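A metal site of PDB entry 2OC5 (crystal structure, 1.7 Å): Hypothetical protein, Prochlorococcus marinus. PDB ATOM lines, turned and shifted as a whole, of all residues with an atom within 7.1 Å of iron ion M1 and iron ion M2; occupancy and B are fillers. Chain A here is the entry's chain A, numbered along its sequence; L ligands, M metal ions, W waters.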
ATOM      1  N   VAL A  42      18.712  -1.967 -22.548  1.00  0.00           N
ATOM      2  CA  VAL A  42      18.096  -1.272 -21.447  1.00  0.00           C
ATOM      3  C   VAL A  42      18.866   0.052 -21.112  1.00  0.00           C
ATOM      4  O   VAL A  42      18.269   1.127 -20.974  1.00  0.00           O
ATOM      5  CB  VAL A  42      18.069  -2.249 -20.242  1.00  0.00           C
ATOM      6  CG1 VAL A  42      17.763  -1.550 -18.966  1.00  0.00           C
ATOM      7  CG2 VAL A  42      17.014  -3.388 -20.530  1.00  0.00           C
ATOM      8  N   GLY A  45      18.169   2.489 -23.838  1.00  0.00           N
ATOM      9  CA  GLY A  45      16.798   2.918 -23.699  1.00  0.00           C
ATOM     10  C   GLY A  45      16.600   3.972 -22.624  1.00  0.00           C
ATOM     11  O   GLY A  45      15.889   4.960 -22.848  1.00  0.00           O
ATOM     12  N   GLU A  46      17.198   3.756 -21.469  1.00  0.00           N
ATOM     13  CA  GLU A  46      17.127   4.744 -20.382  1.00  0.00           C
ATOM     14  C   GLU A  46      17.774   6.093 -20.779  1.00  0.00           C
ATOM     15  O   GLU A  46      17.208   7.152 -20.547  1.00  0.00           O
ATOM     16  CB  GLU A  46      17.721   4.197 -19.069  1.00  0.00           C
ATOM     17  CG  GLU A  46      17.178   2.850 -18.585  1.00  0.00           C
ATOM     18  CD  GLU A  46      15.749   2.834 -18.097  1.00  0.00           C
ATOM     19  OE1 GLU A  46      15.223   3.914 -17.884  1.00  0.00           O
ATOM     20  OE2 GLU A  46      15.160   1.713 -17.909  1.00  0.00           O
ATOM     21  N   ALA A  49      15.464   7.794 -23.250  1.00  0.00           N
ATOM     22  CA  ALA A  49      14.291   8.286 -22.532  1.00  0.00           C
ATOM     23  C   ALA A  49      14.612   9.626 -21.870  1.00  0.00           C
ATOM     24  O   ALA A  49      13.821  10.585 -21.988  1.00  0.00           O
ATOM     25  CB  ALA A  49      13.877   7.253 -21.515  1.00  0.00           C
ATOM     26  N   HIS A  50      15.749   9.706 -21.154  1.00  0.00           N
ATOM     27  CA  HIS A  50      16.248  10.984 -20.694  1.00  0.00           C
ATOM     28  C   HIS A  50      16.255  12.049 -21.770  1.00  0.00           C
ATOM     29  O   HIS A  50      15.720  13.172 -21.582  1.00  0.00           O
ATOM     30  CB  HIS A  50      17.655  10.840 -20.095  1.00  0.00           C
ATOM     31  CG  HIS A  50      18.346  12.143 -19.866  1.00  0.00           C
ATOM     32  ND1 HIS A  50      18.997  12.823 -20.881  1.00  0.00           N
ATOM     33  CD2 HIS A  50      18.451  12.932 -18.761  1.00  0.00           C
ATOM     34  CE1 HIS A  50      19.490  13.952 -20.392  1.00  0.00           C
ATOM     35  NE2 HIS A  50      19.146  14.050 -19.109  1.00  0.00           N
ATOM     36  N   TYR A  53      12.629  13.099 -22.943  1.00  0.00           N
ATOM     37  CA  TYR A  53      11.835  13.968 -22.062  1.00  0.00           C
ATOM     38  C   TYR A  53      12.383  15.397 -22.082  1.00  0.00           C
ATOM     39  O   TYR A  53      11.612  16.363 -22.155  1.00  0.00           O
ATOM     40  CB  TYR A  53      11.731  13.342 -20.619  1.00  0.00           C
ATOM     41  CG  TYR A  53      10.737  12.151 -20.571  1.00  0.00           C
ATOM     42  CD1 TYR A  53       9.414  12.306 -21.016  1.00  0.00           C
ATOM     43  CD2 TYR A  53      11.118  10.879 -20.118  1.00  0.00           C
ATOM     44  CE1 TYR A  53       8.505  11.223 -21.030  1.00  0.00           C
ATOM     45  CE2 TYR A  53      10.245   9.801 -20.130  1.00  0.00           C
ATOM     46  CZ  TYR A  53       8.916   9.960 -20.582  1.00  0.00           C
ATOM     47  OH  TYR A  53       8.079   8.861 -20.593  1.00  0.00           O
ATOM     48  N   LEU A  70      11.400  13.810 -14.684  1.00  0.00           N
ATOM     49  CA  LEU A  70      11.268  12.488 -15.347  1.00  0.00           C
ATOM     50  C   LEU A  70      12.631  12.066 -15.935  1.00  0.00           C
ATOM     51  O   LEU A  70      13.065  10.917 -15.738  1.00  0.00           O
ATOM     52  CB  LEU A  70      10.180  12.470 -16.440  1.00  0.00           C
ATOM     53  CG  LEU A  70       8.765  12.848 -16.023  1.00  0.00           C
ATOM     54  CD1 LEU A  70       7.770  12.693 -17.148  1.00  0.00           C
ATOM     55  CD2 LEU A  70       8.306  12.121 -14.751  1.00  0.00           C
ATOM     56  N   MET A  73      14.977  10.794 -13.359  1.00  0.00           N
ATOM     57  CA  MET A  73      14.637   9.396 -13.018  1.00  0.00           C
ATOM     58  C   MET A  73      15.270   8.433 -14.024  1.00  0.00           C
ATOM     59  O   MET A  73      15.758   7.364 -13.636  1.00  0.00           O
ATOM     60  CB  MET A  73      13.138   9.163 -12.994  1.00  0.00           C
ATOM     61  CG  MET A  73      12.419   9.965 -11.959  1.00  0.00           C
ATOM     62  SD  MET A  73      10.419   9.526 -11.963  1.00  0.00           S
ATOM     63  CE  MET A  73       9.791  11.389 -11.355  1.00  0.00           C
ATOM     64  N   GLU A  74      15.203   8.762 -15.307  1.00  0.00           N
ATOM     65  CA  GLU A  74      15.761   7.868 -16.337  1.00  0.00           C
ATOM     66  C   GLU A  74      17.256   7.677 -16.129  1.00  0.00           C
ATOM     67  O   GLU A  74      17.777   6.579 -16.319  1.00  0.00           O
ATOM     68  CB  GLU A  74      15.492   8.391 -17.720  1.00  0.00           C
ATOM     69  CG  GLU A  74      13.997   8.559 -18.100  1.00  0.00           C
ATOM     70  CD  GLU A  74      13.199   7.291 -18.161  1.00  0.00           C
ATOM     71  OE1 GLU A  74      13.716   6.192 -17.845  1.00  0.00           O
ATOM     72  OE2 GLU A  74      12.017   7.392 -18.556  1.00  0.00           O
ATOM     73  N   MET A  75      17.964   8.726 -15.740  1.00  0.00           N
ATOM     74  CA  MET A  75      19.405   8.590 -15.482  1.00  0.00           C
ATOM     75  C   MET A  75      19.706   7.710 -14.289  1.00  0.00           C
ATOM     76  O   MET A  75      20.693   6.976 -14.281  1.00  0.00           O
ATOM     77  CB  MET A  75      20.090   9.946 -15.358  1.00  0.00           C
ATOM     78  CG  MET A  75      20.065  10.737 -16.663  1.00  0.00           C
ATOM     79  SD  MET A  75      20.774   9.832 -18.288  1.00  0.00           S
ATOM     80  CE  MET A  75      22.587   9.754 -17.627  1.00  0.00           C
ATOM     81  N   HIS A  77      17.703   5.216 -13.456  1.00  0.00           N
ATOM     82  CA  HIS A  77      17.442   3.886 -14.017  1.00  0.00           C
ATOM     83  C   HIS A  77      18.717   3.399 -14.773  1.00  0.00           C
ATOM     84  O   HIS A  77      19.152   2.257 -14.617  1.00  0.00           O
ATOM     85  CB  HIS A  77      16.254   3.868 -15.012  1.00  0.00           C
ATOM     86  CG  HIS A  77      14.944   4.319 -14.436  1.00  0.00           C
ATOM     87  ND1 HIS A  77      13.822   4.585 -15.225  1.00  0.00           N
ATOM     88  CD2 HIS A  77      14.562   4.470 -13.147  1.00  0.00           C
ATOM     89  CE1 HIS A  77      12.817   4.920 -14.412  1.00  0.00           C
ATOM     90  NE2 HIS A  77      13.250   4.863 -13.151  1.00  0.00           N
ATOM     91  N   LYS A  78      19.280   4.280 -15.605  1.00  0.00           N
ATOM     92  CA  LYS A  78      20.456   3.938 -16.407  1.00  0.00           C
ATOM     93  C   LYS A  78      21.600   3.513 -15.518  1.00  0.00           C
ATOM     94  O   LYS A  78      22.293   2.514 -15.805  1.00  0.00           O
ATOM     95  CB  LYS A  78      20.880   5.129 -17.262  1.00  0.00           C
ATOM     96  CG  LYS A  78      21.955   4.777 -18.274  1.00  0.00           C
ATOM     97  CD  LYS A  78      22.627   6.034 -18.864  1.00  0.00           C
ATOM     98  CE  LYS A  78      23.643   5.607 -19.972  1.00  0.00           C
ATOM     99  NZ  LYS A  78      24.445   6.767 -20.456  1.00  0.00           N
ATOM    100  N   PHE A  81      20.855  -0.075 -14.004  1.00  0.00           N
ATOM    101  CA  PHE A  81      21.000  -1.165 -14.956  1.00  0.00           C
ATOM    102  C   PHE A  81      22.452  -1.354 -15.418  1.00  0.00           C
ATOM    103  O   PHE A  81      22.873  -2.450 -15.681  1.00  0.00           O
ATOM    104  CB  PHE A  81      20.029  -1.009 -16.125  1.00  0.00           C
ATOM    105  CG  PHE A  81      18.585  -1.161 -15.709  1.00  0.00           C
ATOM    106  CD1 PHE A  81      18.163  -2.315 -15.005  1.00  0.00           C
ATOM    107  CD2 PHE A  81      17.628  -0.224 -16.033  1.00  0.00           C
ATOM    108  CE1 PHE A  81      16.835  -2.497 -14.660  1.00  0.00           C
ATOM    109  CE2 PHE A  81      16.284  -0.415 -15.681  1.00  0.00           C
ATOM    110  CZ  PHE A  81      15.911  -1.532 -14.965  1.00  0.00           C
ATOM    111  N   GLN A 124       7.375   7.924 -26.835  1.00  0.00           N
ATOM    112  CA  GLN A 124       8.124   7.763 -25.571  1.00  0.00           C
ATOM    113  C   GLN A 124       7.246   7.359 -24.398  1.00  0.00           C
ATOM    114  O   GLN A 124       7.504   6.354 -23.736  1.00  0.00           O
ATOM    115  CB  GLN A 124       8.931   9.005 -25.201  1.00  0.00           C
ATOM    116  CG  GLN A 124       9.663   8.893 -23.821  1.00  0.00           C
ATOM    117  CD  GLN A 124      10.668   7.746 -23.695  1.00  0.00           C
ATOM    118  OE1 GLN A 124      11.517   7.588 -24.557  1.00  0.00           O
ATOM    119  NE2 GLN A 124      10.518   6.892 -22.629  1.00  0.00           N
ATOM    120  N   ILE A 128       7.056   3.146 -25.575  1.00  0.00           N
ATOM    121  CA  ILE A 128       8.314   2.739 -24.958  1.00  0.00           C
ATOM    122  C   ILE A 128       8.127   2.439 -23.461  1.00  0.00           C
ATOM    123  O   ILE A 128       8.669   1.474 -22.982  1.00  0.00           O
ATOM    124  CB  ILE A 128       9.482   3.716 -25.254  1.00  0.00           C
ATOM    125  CG1 ILE A 128       9.829   3.707 -26.758  1.00  0.00           C
ATOM    126  CG2 ILE A 128      10.737   3.296 -24.484  1.00  0.00           C
ATOM    127  CD1 ILE A 128      10.680   4.921 -27.236  1.00  0.00           C
ATOM    128  N   GLU A 129       7.371   3.248 -22.763  1.00  0.00           N
ATOM    129  CA  GLU A 129       7.110   2.957 -21.329  1.00  0.00           C
ATOM    130  C   GLU A 129       6.368   1.625 -21.175  1.00  0.00           C
ATOM    131  O   GLU A 129       6.687   0.853 -20.275  1.00  0.00           O
ATOM    132  CB  GLU A 129       6.377   4.090 -20.639  1.00  0.00           C
ATOM    133  CG  GLU A 129       7.099   5.486 -20.594  1.00  0.00           C
ATOM    134  CD  GLU A 129       8.414   5.543 -19.795  1.00  0.00           C
ATOM    135  OE1 GLU A 129       8.728   4.596 -19.014  1.00  0.00           O
ATOM    136  OE2 GLU A 129       9.065   6.597 -19.931  1.00  0.00           O
ATOM    137  N   ALA A 132       8.905  -1.164 -21.768  1.00  0.00           N
ATOM    138  CA  ALA A 132       9.775  -1.289 -20.596  1.00  0.00           C
ATOM    139  C   ALA A 132       9.106  -1.973 -19.425  1.00  0.00           C
ATOM    140  O   ALA A 132       9.645  -2.878 -18.791  1.00  0.00           O
ATOM    141  CB  ALA A 132      10.273   0.076 -20.168  1.00  0.00           C
ATOM    142  N   TYR A 136      10.394  -5.407 -17.822  1.00  0.00           N
ATOM    143  CA  TYR A 136      10.822  -5.395 -16.400  1.00  0.00           C
ATOM    144  C   TYR A 136       9.942  -6.332 -15.540  1.00  0.00           C
ATOM    145  O   TYR A 136      10.465  -7.100 -14.722  1.00  0.00           O
ATOM    146  CB  TYR A 136      10.969  -3.981 -15.807  1.00  0.00           C
ATOM    147  CG  TYR A 136      11.999  -3.101 -16.524  1.00  0.00           C
ATOM    148  CD1 TYR A 136      13.001  -3.687 -17.288  1.00  0.00           C
ATOM    149  CD2 TYR A 136      11.899  -1.765 -16.552  1.00  0.00           C
ATOM    150  CE1 TYR A 136      13.896  -2.948 -17.979  1.00  0.00           C
ATOM    151  CE2 TYR A 136      12.801  -1.001 -17.277  1.00  0.00           C
ATOM    152  CZ  TYR A 136      13.784  -1.592 -17.985  1.00  0.00           C
ATOM    153  OH  TYR A 136      14.735  -0.848 -18.706  1.00  0.00           O
ATOM    154  N   VAL A 154      12.519   0.340 -10.209  1.00  0.00           N
ATOM    155  CA  VAL A 154      12.196   1.041 -11.437  1.00  0.00           C
ATOM    156  C   VAL A 154      10.715   0.964 -11.923  1.00  0.00           C
ATOM    157  O   VAL A 154      10.215   1.871 -12.602  1.00  0.00           O
ATOM    158  CB  VAL A 154      13.133   0.442 -12.515  1.00  0.00           C
ATOM    159  CG1 VAL A 154      12.727   0.810 -13.937  1.00  0.00           C
ATOM    160  CG2 VAL A 154      14.591   0.816 -12.230  1.00  0.00           C
ATOM    161  N   ASP A 157       8.251   3.775 -11.261  1.00  0.00           N
ATOM    162  CA  ASP A 157       8.515   4.988 -12.043  1.00  0.00           C
ATOM    163  C   ASP A 157       7.928   4.902 -13.465  1.00  0.00           C
ATOM    164  O   ASP A 157       7.545   5.933 -14.051  1.00  0.00           O
ATOM    165  CB  ASP A 157      10.019   5.213 -12.190  1.00  0.00           C
ATOM    166  CG  ASP A 157      10.685   5.700 -10.903  1.00  0.00           C
ATOM    167  OD1 ASP A 157       9.965   6.023  -9.931  1.00  0.00           O
ATOM    168  OD2 ASP A 157      11.944   5.773 -10.911  1.00  0.00           O
ATOM    169  N   GLU A 158       7.896   3.700 -14.050  1.00  0.00           N
ATOM    170  CA  GLU A 158       7.331   3.494 -15.407  1.00  0.00           C
ATOM    171  C   GLU A 158       5.872   3.935 -15.404  1.00  0.00           C
ATOM    172  O   GLU A 158       5.412   4.593 -16.314  1.00  0.00           O
ATOM    173  CB  GLU A 158       7.401   2.035 -15.862  1.00  0.00           C
ATOM    174  CG  GLU A 158       8.724   1.335 -15.596  1.00  0.00           C
ATOM    175  CD  GLU A 158       9.892   2.032 -16.209  1.00  0.00           C
ATOM    176  OE1 GLU A 158      10.163   3.189 -15.835  1.00  0.00           O
ATOM    177  OE2 GLU A 158      10.549   1.444 -17.090  1.00  0.00           O
ATOM    178  N   HIS A 161       5.588   7.582 -15.536  1.00  0.00           N
ATOM    179  CA  HIS A 161       5.860   8.088 -16.919  1.00  0.00           C
ATOM    180  C   HIS A 161       4.678   7.851 -17.839  1.00  0.00           C
ATOM    181  O   HIS A 161       4.244   8.751 -18.563  1.00  0.00           O
ATOM    182  CB  HIS A 161       7.116   7.468 -17.484  1.00  0.00           C
ATOM    183  CG  HIS A 161       8.331   7.811 -16.684  1.00  0.00           C
ATOM    184  ND1 HIS A 161       9.550   7.224 -16.895  1.00  0.00           N
ATOM    185  CD2 HIS A 161       8.456   8.571 -15.570  1.00  0.00           C
ATOM    186  CE1 HIS A 161      10.425   7.714 -16.024  1.00  0.00           C
ATOM    187  NE2 HIS A 161       9.777   8.500 -15.187  1.00  0.00           N
ATOM    188  N   LEU A 162       4.162   6.627 -17.835  1.00  0.00           N
ATOM    189  CA  LEU A 162       2.923   6.342 -18.549  1.00  0.00           C
ATOM    190  C   LEU A 162       1.787   7.299 -18.178  1.00  0.00           C
ATOM    191  O   LEU A 162       1.106   7.835 -19.038  1.00  0.00           O
ATOM    192  CB  LEU A 162       2.461   4.939 -18.210  1.00  0.00           C
ATOM    193  CG  LEU A 162       3.074   3.761 -18.915  1.00  0.00           C
ATOM    194  CD1 LEU A 162       2.665   2.562 -18.062  1.00  0.00           C
ATOM    195  CD2 LEU A 162       2.528   3.599 -20.360  1.00  0.00           C
HETATM  196  O1  LIG L   1      13.105   3.738 -19.414  1.00  0.00           O
HETATM  197  O2  LIG L   1      12.364   3.957 -20.332  1.00  0.00           O
HETATM  198  O3  LIG L   1      11.485   4.816 -20.265  1.00  0.00           O
HETATM  199  O4  LIG L   1      12.556   3.147 -21.583  1.00  0.00           O
HETATM  200  O5  LIG L   1      13.553   2.023 -21.522  1.00  0.00           O
HETATM  201  C1  LIG L   1      13.410   1.098 -22.723  1.00  0.00           C
HETATM  202  C2  LIG L   1      13.988  -0.280 -22.457  1.00  0.00           C
HETATM  203  C3  LIG L   1      13.350  -1.361 -23.328  1.00  0.00           C
HETATM  204  O6  LIG L   1      13.927  -2.723 -22.950  1.00  0.00           O
HETATM  205  O7  LIG L   1      13.516  -3.845 -23.906  1.00  0.00           O
HETATM  206  O8  LIG L   1      14.436  -5.062 -23.752  1.00  0.00           O
HETATM  207  O9  LIG L   1      13.718  -6.376 -23.433  1.00  0.00           O
HETATM  208  O10 LIG L   1      14.335  -7.236 -22.303  1.00  0.00           O
HETATM  209  O11 LIG L   1      14.813  -6.478 -21.081  1.00  0.00           O
HETATM  210  O12 LIG L   1      14.812  -7.277 -19.788  1.00  0.00           O
HETATM  211  O13 LIG L   1      15.209  -6.421 -18.596  1.00  0.00           O
HETATM  212  O14 LIG L   1      16.687  -6.587 -18.273  1.00  0.00           O
HETATM  213  O15 LIG L   1      17.058  -5.576 -17.193  1.00  0.00           O
HETATM  214  O16 LIG L   1      18.529  -5.670 -16.834  1.00  0.00           O
HETATM  215  O17 LIG L   1      19.454  -4.940 -17.743  1.00  0.00           O
HETATM  216 FE    FE M   1      13.235   4.315 -17.379  1.00  0.00          FE
HETATM  217 FE    FE M   2      10.586   5.833 -18.457  1.00  0.00          FE
HETATM  218  O   HOH W   1      12.892   2.406 -16.891  1.00  0.00           O
HETATM  219  O   HOH W   2      11.401   4.765 -16.958  1.00  0.00           O
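The side-chain sulfur of Met 73 sits at hydrogen-bond distance from a ring nitrogen (NE2) of His 161 (3.4 Å). OE2 of Glu 129 lies close to OH of Tyr 53 (2.6 Å). The backbone carbonyl oxygen (O) of Gln 124 lies within hydrogen-bond range of the backbone NH (N) of Glu 129 (3.3 Å). OE2 of Glu 46 lies within hydrogen-bond range of OH of Tyr 136. NE2 of His 77 lies within hydrogen-bond range of OD2 of Asp 157 (2.7 Å).
Residues that only touch iron ion M1: Glu 158. The nearest printed residue that does not touch iron ion M1 is His 161 (4.6 Å).
Residues that only touch iron ion M2: Glu 158. The nearest printed residue that does not touch iron ion M2 is Gln 124 (4.3 Å).
Iron ion M1 is bound by water W2, the side-chain carboxylate (OE1) of Glu 74, water W1, the side-chain carboxylate (OE1) of Glu 46, an oxygen (O1) of the ligand and a ring nitrogen (ND1) of His 77.
Iron ion M2 is bound by water W2, at 2.0 Å. OE2 of Glu 74 binds iron ion M2, at 2.1 Å. The side-chain carboxylate (OE2) of Glu 129 is bound to iron ion M2 (2.3 Å). O3 of the ligand is bound to iron ion M2, at 2.3 Å. OE1 of Glu 129 is bound to iron ion M2. ND1 of His 161 is bound to iron ion M2 (2.3 Å).
Water W1 lies within hydrogen-bond range of the side-chain carboxylate of Glu 158 (2.5 Å) and the side-chain carboxylate of Glu 46 (2.6 Å).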
